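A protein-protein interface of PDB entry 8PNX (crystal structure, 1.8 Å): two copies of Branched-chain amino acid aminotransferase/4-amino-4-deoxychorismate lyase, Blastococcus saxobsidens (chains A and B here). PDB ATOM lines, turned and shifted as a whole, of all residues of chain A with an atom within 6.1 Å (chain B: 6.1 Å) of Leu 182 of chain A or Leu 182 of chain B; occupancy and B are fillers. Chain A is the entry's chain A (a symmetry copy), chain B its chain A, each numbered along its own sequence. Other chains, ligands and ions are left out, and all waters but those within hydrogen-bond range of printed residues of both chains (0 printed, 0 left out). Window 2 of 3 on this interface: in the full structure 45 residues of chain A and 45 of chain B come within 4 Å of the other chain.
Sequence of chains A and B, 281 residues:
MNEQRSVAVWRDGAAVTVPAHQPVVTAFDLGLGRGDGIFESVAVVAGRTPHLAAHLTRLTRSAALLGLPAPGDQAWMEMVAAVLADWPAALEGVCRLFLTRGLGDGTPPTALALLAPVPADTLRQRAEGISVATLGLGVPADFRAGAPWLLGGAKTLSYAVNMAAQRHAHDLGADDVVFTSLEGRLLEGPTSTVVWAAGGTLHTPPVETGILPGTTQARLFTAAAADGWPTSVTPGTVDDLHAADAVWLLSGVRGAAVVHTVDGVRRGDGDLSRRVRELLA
O of Gly 138 of chain B sits close to O of Gly 138 of chain A (3.2 Å).
O of Thr 180 of chain A sits at hydrogen-bond distance from N of Leu 137 of chain A (2.9 Å). N of Leu 137 of chain B lies within hydrogen-bond range of O of Thr 180 of chain B, at 2.9 Å. The backbone carbonyl oxygen (O) of Val 139 of chain A lies within hydrogen-bond range of the backbone NH (N) of Leu 182 of chain A. O of Val 139 of chain B lies within hydrogen-bond range of N of Leu 182 of chain B (2.9 Å).
O of Leu 137 of chain A touches CG1 of Val 139 of chain B, at 3.98 Å. CE2 of Phe 143 of chain B touches C of Leu 137 of chain A, 3.8 Å away. Gly 138 of chain A touches Val 139 of chain B. Pro 140 of chain B touches Gly 138 of chain A. Gly 138 of chain A touches Phe 143 of chain B (CA to CZ, 3.5 Å). Leu 137 of chain B touches Val 139 of chain A. Gly 138 of chain B touches Val 139 of chain A. Gly 138 of chain B touches Pro 140 of chain A (O to CD, 3.0 Å). Phe 143 of chain A touches Leu 137 of chain B (CE2 to C, 3.8 Å). CA of Gly 138 of chain B touches CZ of Phe 143 of chain A (3.5 Å).
Leu 182 of chain A touches just these residues of chain B: Pro 140 and Leu 182. Leu 182 of chain B touches just these residues of chain A: Pro 140 and Leu 182. Printed residues of chain B within 4 Å of Gly 138 of chain A: Gly 138, Val 139, Pro 140 and Phe 143. Of the printed residues of chain A, Gly 138 of chain B touches Gly 138, Val 139, Pro 140 and Phe 143. Of the printed residues of chain A, Phe 143 of chain B touches Leu 137 and Gly 138. Printed residues of chain A within 4 Å of Pro 140 of chain B: Gly 138 (3.0 Å) and Leu 182 (3.7 Å). Printed residues of chain B within 4 Å of Val 139 of chain A: Leu 137, Gly 138 and Val 139. Gly 184 of chain A touches none of the printed residues of chain B. Ala 141 of chain B touches none of the printed residues of chain A.
Hydrophobic or aromatic side chains of chain B within 4 Å of the printed part of chain A: Val 139, Pro 140, Phe 143 and Leu 182. Hydrophobic or aromatic side chains of chain A within 4 Å of the printed part of chain B: Val 139, Pro 140, Phe 143 and Leu 182. Among the printed residues, 15 pairs touch across the chains.
Gly 138 of chain A touches its own counterpart, Gly 138 of chain B. Gly 138 of chain A touches Phe 143 of chain B, and with the chains exchanged Phe 143 of chain A touches Gly 138 of chain B. Pro 140 of chain A touches Leu 182 of chain B, and with the chains exchanged Leu 182 of chain A touches Pro 140 of chain B. Leu 182 of chain B touches its own counterpart, Leu 182 of chain A. Positions printed for both chains: 137, 138, 139, 140, 141, 143, 180, 181, 182, 183, 184 and 185.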
ATOM      1  N   LEU A 137     -17.507  12.754  22.088  1.00  0.00           N
ATOM      2  CA  LEU A 137     -18.404  12.128  21.069  1.00  0.00           C
ATOM      3  C   LEU A 137     -19.872  12.227  21.515  1.00  0.00           C
ATOM      4  O   LEU A 137     -20.750  12.067  20.641  1.00  0.00           O
ATOM      5  CB  LEU A 137     -18.010  10.656  20.903  1.00  0.00           C
ATOM      6  CG  LEU A 137     -17.450  10.261  19.539  1.00  0.00           C
ATOM      7  CD1 LEU A 137     -16.795  11.442  18.827  1.00  0.00           C
ATOM      8  CD2 LEU A 137     -16.473   9.111  19.675  1.00  0.00           C
ATOM      9  N   GLY A 138     -20.117  12.373  22.824  1.00  0.00           N
ATOM     10  CA  GLY A 138     -21.451  12.458  23.437  1.00  0.00           C
ATOM     11  C   GLY A 138     -22.145  11.110  23.519  1.00  0.00           C
ATOM     12  O   GLY A 138     -23.314  11.065  23.853  1.00  0.00           O
ATOM     13  N   VAL A 139     -21.448  10.024  23.229  1.00  0.00           N
ATOM     14  CA  VAL A 139     -22.043   8.673  23.394  1.00  0.00           C
ATOM     15  C   VAL A 139     -21.560   8.124  24.726  1.00  0.00           C
ATOM     16  O   VAL A 139     -20.389   8.214  25.008  1.00  0.00           O
ATOM     17  CB  VAL A 139     -21.645   7.738  22.251  1.00  0.00           C
ATOM     18  CG1 VAL A 139     -22.214   8.250  20.942  1.00  0.00           C
ATOM     19  CG2 VAL A 139     -20.124   7.573  22.211  1.00  0.00           C
ATOM     20  N   PRO A 140     -22.415   7.467  25.525  1.00  0.00           N
ATOM     21  CA  PRO A 140     -21.935   6.758  26.711  1.00  0.00           C
ATOM     22  C   PRO A 140     -20.967   5.628  26.310  1.00  0.00           C
ATOM     23  O   PRO A 140     -21.042   5.051  25.217  1.00  0.00           O
ATOM     24  CB  PRO A 140     -23.204   6.274  27.414  1.00  0.00           C
ATOM     25  CG  PRO A 140     -24.362   6.972  26.701  1.00  0.00           C
ATOM     26  CD  PRO A 140     -23.860   7.364  25.339  1.00  0.00           C
ATOM     27  N   ALA A 141     -19.986   5.366  27.176  1.00  0.00           N
ATOM     28  CA  ALA A 141     -18.914   4.367  26.961  1.00  0.00           C
ATOM     29  C   ALA A 141     -19.486   2.969  26.618  1.00  0.00           C
ATOM     30  O   ALA A 141     -18.909   2.317  25.714  1.00  0.00           O
ATOM     31  CB  ALA A 141     -18.044   4.352  28.196  1.00  0.00           C
ATOM     32  N   PHE A 143     -22.547   2.311  25.302  1.00  0.00           N
ATOM     33  CA  PHE A 143     -23.655   2.399  24.322  1.00  0.00           C
ATOM     34  C   PHE A 143     -23.373   1.583  23.055  1.00  0.00           C
ATOM     35  O   PHE A 143     -24.315   0.848  22.606  1.00  0.00           O
ATOM     36  CB  PHE A 143     -24.025   3.837  23.959  1.00  0.00           C
ATOM     37  CG  PHE A 143     -25.349   3.921  23.230  1.00  0.00           C
ATOM     38  CD1 PHE A 143     -26.558   3.998  23.933  1.00  0.00           C
ATOM     39  CD2 PHE A 143     -25.397   3.848  21.845  1.00  0.00           C
ATOM     40  CE1 PHE A 143     -27.766   4.012  23.263  1.00  0.00           C
ATOM     41  CE2 PHE A 143     -26.615   3.847  21.180  1.00  0.00           C
ATOM     42  CZ  PHE A 143     -27.791   3.927  21.888  1.00  0.00           C
ATOM     43  N   THR A 180     -13.621  11.449  23.826  1.00  0.00           N
ATOM     44  CA  THR A 180     -14.104  11.006  25.155  1.00  0.00           C
ATOM     45  C   THR A 180     -15.576  10.636  25.069  1.00  0.00           C
ATOM     46  O   THR A 180     -16.370  11.240  24.257  1.00  0.00           O
ATOM     47  CB  THR A 180     -13.880  12.057  26.252  1.00  0.00           C
ATOM     48  OG1 THR A 180     -14.622  13.240  25.906  1.00  0.00           O
ATOM     49  CG2 THR A 180     -12.412  12.366  26.419  1.00  0.00           C
ATOM     50  N   SER A 181     -15.966   9.671  25.878  1.00  0.00           N
ATOM     51  CA  SER A 181     -17.389   9.297  26.041  1.00  0.00           C
ATOM     52  C   SER A 181     -18.159  10.388  26.806  1.00  0.00           C
ATOM     53  O   SER A 181     -17.537  11.351  27.365  1.00  0.00           O
ATOM     54  CB  SER A 181     -17.430   7.974  26.780  1.00  0.00           C
ATOM     55  OG  SER A 181     -17.165   8.242  28.165  1.00  0.00           O
ATOM     56  N   LEU A 182     -19.474  10.203  26.944  1.00  0.00           N
ATOM     57  CA  LEU A 182     -20.360  11.212  27.579  1.00  0.00           C
ATOM     58  C   LEU A 182     -19.914  11.481  29.024  1.00  0.00           C
ATOM     59  O   LEU A 182     -19.900  12.681  29.392  1.00  0.00           O
ATOM     60  CB  LEU A 182     -21.804  10.704  27.483  1.00  0.00           C
ATOM     61  CG  LEU A 182     -22.881  11.657  27.983  1.00  0.00           C
ATOM     62  CD1 LEU A 182     -22.858  12.971  27.207  1.00  0.00           C
ATOM     63  CD2 LEU A 182     -24.258  11.006  27.900  1.00  0.00           C
ATOM     64  N   GLU A 183     -19.546  10.418  29.755  1.00  0.00           N
ATOM     65  CA  GLU A 183     -19.073  10.407  31.170  1.00  0.00           C
ATOM     66  C   GLU A 183     -17.590  10.775  31.285  1.00  0.00           C
ATOM     67  O   GLU A 183     -17.113  10.734  32.386  1.00  0.00           O
ATOM     68  CB  GLU A 183     -19.096   9.012  31.824  1.00  0.00           C
ATOM     69  CG  GLU A 183     -20.349   8.212  31.634  1.00  0.00           C
ATOM     70  CD  GLU A 183     -20.414   7.292  30.432  1.00  0.00           C
ATOM     71  OE1 GLU A 183     -19.571   7.402  29.479  1.00  0.00           O
ATOM     72  OE2 GLU A 183     -21.410   6.518  30.426  1.00  0.00           O
ATOM     73  N   GLY A 184     -16.862  11.040  30.192  1.00  0.00           N
ATOM     74  CA  GLY A 184     -15.464  11.502  30.225  1.00  0.00           C
ATOM     75  C   GLY A 184     -14.450  10.376  30.098  1.00  0.00           C
ATOM     76  O   GLY A 184     -13.256  10.677  30.248  1.00  0.00           O
ATOM     77  N   ARG A 185     -14.880   9.163  29.715  1.00  0.00           N
ATOM     78  CA  ARG A 185     -13.938   8.039  29.470  1.00  0.00           C
ATOM     79  C   ARG A 185     -13.156   8.276  28.164  1.00  0.00           C
ATOM     80  O   ARG A 185     -13.735   8.726  27.141  1.00  0.00           O
ATOM     81  CB  ARG A 185     -14.677   6.696  29.564  1.00  0.00           C
ATOM     82  CG  ARG A 185     -14.732   6.138  30.984  1.00  0.00           C
ATOM     83  CD  ARG A 185     -15.756   5.062  31.334  1.00  0.00           C
ATOM     84  NE  ARG A 185     -15.823   3.645  30.879  1.00  0.00           N
ATOM     85  CZ  ARG A 185     -15.030   2.938  30.042  1.00  0.00           C
ATOM     86  NH1 ARG A 185     -13.948   3.434  29.465  1.00  0.00           N
ATOM     87  NH2 ARG A 185     -15.348   1.670  29.799  1.00  0.00           N
ATOM     88  N   LEU B 137     -29.226   6.743  18.624  1.00  0.00           N
ATOM     89  CA  LEU B 137     -27.877   7.281  18.267  1.00  0.00           C
ATOM     90  C   LEU B 137     -26.961   7.289  19.503  1.00  0.00           C
ATOM     91  O   LEU B 137     -25.731   7.381  19.305  1.00  0.00           O
ATOM     92  CB  LEU B 137     -28.041   8.707  17.733  1.00  0.00           C
ATOM     93  CG  LEU B 137     -27.671   8.921  16.267  1.00  0.00           C
ATOM     94  CD1 LEU B 137     -27.824   7.642  15.448  1.00  0.00           C
ATOM     95  CD2 LEU B 137     -28.496  10.042  15.666  1.00  0.00           C
ATOM     96  N   GLY B 138     -27.542   7.305  20.709  1.00  0.00           N
ATOM     97  CA  GLY B 138     -26.833   7.342  21.997  1.00  0.00           C
ATOM     98  C   GLY B 138     -26.271   8.716  22.317  1.00  0.00           C
ATOM     99  O   GLY B 138     -25.524   8.842  23.270  1.00  0.00           O
ATOM    100  N   VAL B 139     -26.620   9.734  21.548  1.00  0.00           N
ATOM    101  CA  VAL B 139     -26.187  11.116  21.876  1.00  0.00           C
ATOM    102  C   VAL B 139     -27.342  11.796  22.591  1.00  0.00           C
ATOM    103  O   VAL B 139     -28.456  11.696  22.135  1.00  0.00           O
ATOM    104  CB  VAL B 139     -25.796  11.897  20.620  1.00  0.00           C
ATOM    105  CG1 VAL B 139     -24.585  11.260  19.970  1.00  0.00           C
ATOM    106  CG2 VAL B 139     -26.993  11.999  19.670  1.00  0.00           C
ATOM    107  N   PRO B 140     -27.101  12.573  23.658  1.00  0.00           N
ATOM    108  CA  PRO B 140     -28.161  13.395  24.240  1.00  0.00           C
ATOM    109  C   PRO B 140     -28.661  14.434  23.218  1.00  0.00           C
ATOM    110  O   PRO B 140     -27.934  14.884  22.323  1.00  0.00           O
ATOM    111  CB  PRO B 140     -27.535  14.005  25.496  1.00  0.00           C
ATOM    112  CG  PRO B 140     -26.207  13.274  25.691  1.00  0.00           C
ATOM    113  CD  PRO B 140     -25.822  12.709  24.352  1.00  0.00           C
ATOM    114  N   ALA B 141     -29.954  14.757  23.299  1.00  0.00           N
ATOM    115  CA  ALA B 141     -30.653  15.683  22.379  1.00  0.00           C
ATOM    116  C   ALA B 141     -29.936  17.052  22.282  1.00  0.00           C
ATOM    117  O   ALA B 141     -29.843  17.574  21.144  1.00  0.00           O
ATOM    118  CB  ALA B 141     -32.083  15.807  22.849  1.00  0.00           C
ATOM    119  N   PHE B 143     -26.667  17.671  22.963  1.00  0.00           N
ATOM    120  CA  PHE B 143     -25.199  17.511  22.846  1.00  0.00           C
ATOM    121  C   PHE B 143     -24.646  18.165  21.574  1.00  0.00           C
ATOM    122  O   PHE B 143     -23.594  18.878  21.687  1.00  0.00           O
ATOM    123  CB  PHE B 143     -24.740  16.057  22.941  1.00  0.00           C
ATOM    124  CG  PHE B 143     -23.246  15.939  23.150  1.00  0.00           C
ATOM    125  CD1 PHE B 143     -22.690  15.990  24.435  1.00  0.00           C
ATOM    126  CD2 PHE B 143     -22.386  15.854  22.064  1.00  0.00           C
ATOM    127  CE1 PHE B 143     -21.321  15.944  24.615  1.00  0.00           C
ATOM    128  CE2 PHE B 143     -21.011  15.824  22.253  1.00  0.00           C
ATOM    129  CZ  PHE B 143     -20.485  15.871  23.522  1.00  0.00           C
ATOM    130  N   THR B 180     -33.335   8.091  17.566  1.00  0.00           N
ATOM    131  CA  THR B 180     -33.714   8.703  18.861  1.00  0.00           C
ATOM    132  C   THR B 180     -32.463   9.116  19.619  1.00  0.00           C
ATOM    133  O   THR B 180     -31.365   8.453  19.510  1.00  0.00           O
ATOM    134  CB  THR B 180     -34.582   7.777  19.726  1.00  0.00           C
ATOM    135  OG1 THR B 180     -33.825   6.591  20.024  1.00  0.00           O
ATOM    136  CG2 THR B 180     -35.876   7.434  19.028  1.00  0.00           C
ATOM    137  N   SER B 181     -32.590  10.181  20.384  1.00  0.00           N
ATOM    138  CA  SER B 181     -31.525  10.626  21.312  1.00  0.00           C
ATOM    139  C   SER B 181     -31.398   9.660  22.504  1.00  0.00           C
ATOM    140  O   SER B 181     -32.266   8.745  22.694  1.00  0.00           O
ATOM    141  CB  SER B 181     -31.878  12.026  21.774  1.00  0.00           C
ATOM    142  OG  SER B 181     -32.920  11.910  22.754  1.00  0.00           O
ATOM    143  N   LEU B 182     -30.413   9.910  23.369  1.00  0.00           N
ATOM    144  CA  LEU B 182     -30.112   9.015  24.517  1.00  0.00           C
ATOM    145  C   LEU B 182     -31.336   8.898  25.437  1.00  0.00           C
ATOM    146  O   LEU B 182     -31.610   7.748  25.862  1.00  0.00           O
ATOM    147  CB  LEU B 182     -28.872   9.562  25.234  1.00  0.00           C
ATOM    148  CG  LEU B 182     -28.336   8.715  26.380  1.00  0.00           C
ATOM    149  CD1 LEU B 182     -27.946   7.321  25.898  1.00  0.00           C
ATOM    150  CD2 LEU B 182     -27.152   9.404  27.052  1.00  0.00           C
ATOM    151  N   GLU B 183     -32.024  10.023  25.681  1.00  0.00           N
ATOM    152  CA  GLU B 183     -33.240  10.180  26.530  1.00  0.00           C
ATOM    153  C   GLU B 183     -34.517   9.771  25.789  1.00  0.00           C
ATOM    154  O   GLU B 183     -35.551   9.920  26.382  1.00  0.00           O
ATOM    155  CB  GLU B 183     -33.555  11.641  26.906  1.00  0.00           C
ATOM    156  CG  GLU B 183     -32.403  12.460  27.402  1.00  0.00           C
ATOM    157  CD  GLU B 183     -31.606  13.237  26.375  1.00  0.00           C
ATOM    158  OE1 GLU B 183     -31.727  12.986  25.128  1.00  0.00           O
ATOM    159  OE2 GLU B 183     -30.771  14.043  26.868  1.00  0.00           O
ATOM    160  N   GLY B 184     -34.469   9.354  24.516  1.00  0.00           N
ATOM    161  CA  GLY B 184     -35.632   8.846  23.770  1.00  0.00           C
ATOM    162  C   GLY B 184     -36.332   9.911  22.939  1.00  0.00           C
ATOM    163  O   GLY B 184     -37.393   9.585  22.389  1.00  0.00           O
ATOM    164  N   ARG B 185     -35.713  11.087  22.748  1.00  0.00           N
ATOM    165  CA  ARG B 185     -36.284  12.139  21.866  1.00  0.00           C
ATOM    166  C   ARG B 185     -36.153  11.724  20.389  1.00  0.00           C
ATOM    167  O   ARG B 185     -35.098  11.181  19.965  1.00  0.00           O
ATOM    168  CB  ARG B 185     -35.694  13.511  22.223  1.00  0.00           C
ATOM    169  CG  ARG B 185     -36.467  14.231  23.325  1.00  0.00           C
ATOM    170  CD  ARG B 185     -35.808  15.378  24.085  1.00  0.00           C
ATOM    171  NE  ARG B 185     -35.431  16.734  23.598  1.00  0.00           N
ATOM    172  CZ  ARG B 185     -35.550  17.309  22.380  1.00  0.00           C
ATOM    173  NH1 ARG B 185     -36.100  16.710  21.337  1.00  0.00           N
ATOM    174  NH2 ARG B 185     -35.101  18.552  22.227  1.00  0.00           N
